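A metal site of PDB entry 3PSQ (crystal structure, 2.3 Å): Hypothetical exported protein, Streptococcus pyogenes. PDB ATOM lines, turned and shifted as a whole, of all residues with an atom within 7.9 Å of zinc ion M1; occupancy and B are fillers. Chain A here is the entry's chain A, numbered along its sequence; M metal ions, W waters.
Zinc ion M1 is bound by OD1 of Asp 192 (2.0 Å), ND1 of His 96 (2.1 Å), SG of Cys 190 (2.3 Å) and water W1 (2.3 Å).
O of His 96 is in hydrogen-bond range of ND2 of Asn 100 (3.1 Å). The side-chain carboxylate of Asp 192 sits at hydrogen-bond distance from the side-chain amide nitrogen of Asn 100.
Merely in contact with zinc ion M1: Asn 100 (3.95 Å). Of the 14 residues printed, 4 come within 4 Å of zinc ion M1.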
ATOM      1  N   TYR A  93      17.199  -9.450  18.406  1.00  0.00           N
ATOM      2  CA  TYR A  93      17.282  -8.226  19.183  1.00  0.00           C
ATOM      3  C   TYR A  93      16.164  -8.196  20.239  1.00  0.00           C
ATOM      4  O   TYR A  93      15.131  -8.888  20.099  1.00  0.00           O
ATOM      5  CB  TYR A  93      17.162  -7.010  18.209  1.00  0.00           C
ATOM      6  CG  TYR A  93      17.526  -5.698  18.837  1.00  0.00           C
ATOM      7  CD1 TYR A  93      18.846  -5.325  18.983  1.00  0.00           C
ATOM      8  CD2 TYR A  93      16.516  -4.854  19.336  1.00  0.00           C
ATOM      9  CE1 TYR A  93      19.202  -4.128  19.604  1.00  0.00           C
ATOM     10  CE2 TYR A  93      16.858  -3.661  19.956  1.00  0.00           C
ATOM     11  CZ  TYR A  93      18.196  -3.289  20.085  1.00  0.00           C
ATOM     12  OH  TYR A  93      18.538  -2.096  20.704  1.00  0.00           O
ATOM     13  N   ALA A  94      16.405  -7.440  21.313  1.00  0.00           N
ATOM     14  CA  ALA A  94      15.347  -7.096  22.289  1.00  0.00           C
ATOM     15  C   ALA A  94      15.437  -5.619  22.587  1.00  0.00           C
ATOM     16  O   ALA A  94      16.537  -5.101  22.756  1.00  0.00           O
ATOM     17  CB  ALA A  94      15.446  -7.941  23.589  1.00  0.00           C
ATOM     18  N   HIS A  95      14.295  -4.928  22.582  1.00  0.00           N
ATOM     19  CA  HIS A  95      14.247  -3.550  23.043  1.00  0.00           C
ATOM     20  C   HIS A  95      14.478  -3.476  24.565  1.00  0.00           C
ATOM     21  O   HIS A  95      14.631  -4.499  25.247  1.00  0.00           O
ATOM     22  CB  HIS A  95      12.910  -2.903  22.654  1.00  0.00           C
ATOM     23  CG  HIS A  95      12.835  -2.550  21.199  1.00  0.00           C
ATOM     24  ND1 HIS A  95      13.375  -1.379  20.696  1.00  0.00           N
ATOM     25  CD2 HIS A  95      12.316  -3.210  20.140  1.00  0.00           C
ATOM     26  CE1 HIS A  95      13.176  -1.348  19.384  1.00  0.00           C
ATOM     27  NE2 HIS A  95      12.564  -2.448  19.030  1.00  0.00           N
ATOM     28  N   HIS A  96      14.513  -2.262  25.087  1.00  0.00           N
ATOM     29  CA  HIS A  96      14.922  -2.062  26.467  1.00  0.00           C
ATOM     30  C   HIS A  96      14.226  -2.956  27.489  1.00  0.00           C
ATOM     31  O   HIS A  96      14.896  -3.609  28.303  1.00  0.00           O
ATOM     32  CB  HIS A  96      14.777  -0.583  26.852  1.00  0.00           C
ATOM     33  CG  HIS A  96      14.830  -0.307  28.333  1.00  0.00           C
ATOM     34  ND1 HIS A  96      16.010  -0.189  29.027  1.00  0.00           N
ATOM     35  CD2 HIS A  96      13.840  -0.077  29.232  1.00  0.00           C
ATOM     36  CE1 HIS A  96      15.757   0.095  30.298  1.00  0.00           C
ATOM     37  NE2 HIS A  96      14.442   0.166  30.447  1.00  0.00           N
ATOM     38  N   MET A  97      12.892  -2.985  27.495  1.00  0.00           N
ATOM     39  CA  MET A  97      12.203  -3.818  28.488  1.00  0.00           C
ATOM     40  C   MET A  97      12.445  -5.325  28.305  1.00  0.00           C
ATOM     41  O   MET A  97      12.880  -5.975  29.271  1.00  0.00           O
ATOM     42  CB  MET A  97      10.688  -3.514  28.570  1.00  0.00           C
ATOM     43  CG  MET A  97      10.332  -2.121  29.142  1.00  0.00           C
ATOM     44  SD  MET A  97      10.879  -1.849  30.872  1.00  0.00           S
ATOM     45  CE  MET A  97      10.695  -3.533  31.558  1.00  0.00           C
ATOM     46  N   GLY A  99      14.767  -6.739  26.798  1.00  0.00           N
ATOM     47  CA  GLY A  99      16.162  -7.040  26.967  1.00  0.00           C
ATOM     48  C   GLY A  99      16.487  -7.242  28.439  1.00  0.00           C
ATOM     49  O   GLY A  99      17.135  -8.229  28.809  1.00  0.00           O
ATOM     50  N   ASN A 100      16.057  -6.282  29.276  1.00  0.00           N
ATOM     51  CA  ASN A 100      16.167  -6.411  30.720  1.00  0.00           C
ATOM     52  C   ASN A 100      15.430  -7.650  31.244  1.00  0.00           C
ATOM     53  O   ASN A 100      15.950  -8.339  32.090  1.00  0.00           O
ATOM     54  CB  ASN A 100      15.650  -5.153  31.440  1.00  0.00           C
ATOM     55  CG  ASN A 100      16.732  -4.075  31.593  1.00  0.00           C
ATOM     56  OD1 ASN A 100      17.457  -4.067  32.578  1.00  0.00           O
ATOM     57  ND2 ASN A 100      16.829  -3.171  30.629  1.00  0.00           N
ATOM     58  N   THR A 189      20.964  -6.506  22.871  1.00  0.00           N
ATOM     59  CA  THR A 189      20.046  -5.599  23.489  1.00  0.00           C
ATOM     60  C   THR A 189      20.835  -4.391  24.019  1.00  0.00           C
ATOM     61  O   THR A 189      21.987  -4.196  23.660  1.00  0.00           O
ATOM     62  CB  THR A 189      19.162  -6.298  24.578  1.00  0.00           C
ATOM     63  OG1 THR A 189      18.153  -5.385  25.012  1.00  0.00           O
ATOM     64  CG2 THR A 189      19.995  -6.798  25.754  1.00  0.00           C
ATOM     65  N   CYS A 190      20.180  -3.561  24.838  1.00  0.00           N
ATOM     66  CA  CYS A 190      20.846  -2.428  25.462  1.00  0.00           C
ATOM     67  C   CYS A 190      21.789  -2.835  26.600  1.00  0.00           C
ATOM     68  O   CYS A 190      21.732  -3.941  27.134  1.00  0.00           O
ATOM     69  CB  CYS A 190      19.826  -1.443  25.989  1.00  0.00           C
ATOM     70  SG  CYS A 190      18.730  -2.149  27.248  1.00  0.00           S
ATOM     71  N   GLU A 191      22.667  -1.924  26.967  1.00  0.00           N
ATOM     72  CA  GLU A 191      23.434  -2.060  28.181  1.00  0.00           C
ATOM     73  C   GLU A 191      23.300  -0.720  28.905  1.00  0.00           C
ATOM     74  O   GLU A 191      24.070   0.200  28.643  1.00  0.00           O
ATOM     75  CB  GLU A 191      24.875  -2.410  27.829  1.00  0.00           C
ATOM     76  CG  GLU A 191      25.721  -2.896  28.992  1.00  0.00           C
ATOM     77  CD  GLU A 191      26.735  -3.934  28.535  1.00  0.00           C
ATOM     78  OE1 GLU A 191      27.275  -3.783  27.400  1.00  0.00           O
ATOM     79  OE2 GLU A 191      26.987  -4.904  29.307  1.00  0.00           O
ATOM     80  N   ASP A 192      22.312  -0.611  29.791  1.00  0.00           N
ATOM     81  CA  ASP A 192      21.942   0.684  30.424  1.00  0.00           C
ATOM     82  C   ASP A 192      23.005   1.326  31.340  1.00  0.00           C
ATOM     83  O   ASP A 192      22.746   2.390  31.901  1.00  0.00           O
ATOM     84  CB  ASP A 192      20.639   0.595  31.220  1.00  0.00           C
ATOM     85  CG  ASP A 192      19.485   0.084  30.402  1.00  0.00           C
ATOM     86  OD1 ASP A 192      19.245   0.585  29.260  1.00  0.00           O
ATOM     87  OD2 ASP A 192      18.811  -0.846  30.893  1.00  0.00           O
ATOM     88  N   MET A 193      24.163   0.693  31.502  1.00  0.00           N
ATOM     89  CA  MET A 193      25.194   1.364  32.294  1.00  0.00           C
ATOM     90  C   MET A 193      26.101   2.269  31.476  1.00  0.00           C
ATOM     91  O   MET A 193      26.748   3.132  32.044  1.00  0.00           O
ATOM     92  CB  MET A 193      26.008   0.386  33.139  1.00  0.00           C
ATOM     93  CG  MET A 193      25.197  -0.318  34.245  1.00  0.00           C
ATOM     94  SD  MET A 193      24.485   0.787  35.511  1.00  0.00           S
ATOM     95  CE  MET A 193      22.727   0.745  35.094  1.00  0.00           C
ATOM     96  N   GLY A 197      24.364   2.483  25.215  1.00  0.00           N
ATOM     97  CA  GLY A 197      25.201   1.304  25.120  1.00  0.00           C
ATOM     98  C   GLY A 197      24.439   0.128  24.597  1.00  0.00           C
ATOM     99  O   GLY A 197      23.234  -0.021  24.907  1.00  0.00           O
ATOM    100  N   ARG A 198      25.112  -0.679  23.763  1.00  0.00           N
ATOM    101  CA  ARG A 198      24.524  -1.949  23.276  1.00  0.00           C
ATOM    102  C   ARG A 198      25.488  -3.103  23.502  1.00  0.00           C
ATOM    103  O   ARG A 198      26.695  -2.956  23.365  1.00  0.00           O
ATOM    104  CB  ARG A 198      24.091  -1.896  21.798  1.00  0.00           C
ATOM    105  CG  ARG A 198      23.063  -0.839  21.428  1.00  0.00           C
ATOM    106  CD  ARG A 198      21.663  -1.185  21.889  1.00  0.00           C
ATOM    107  NE  ARG A 198      20.686  -0.154  21.539  1.00  0.00           N
ATOM    108  CZ  ARG A 198      20.299   0.854  22.327  1.00  0.00           C
ATOM    109  NH1 ARG A 198      20.820   0.970  23.555  1.00  0.00           N
ATOM    110  NH2 ARG A 198      19.368   1.731  21.930  1.00  0.00           N
HETATM  111 ZN    ZN M   1      17.873  -0.265  28.162  1.00  0.00          ZN
HETATM  112 ZN    ZN M   2      13.870   0.289  21.548  1.00  0.00          ZN
HETATM  113  O   HOH W   1      17.837   1.541  26.796  1.00  0.00           O
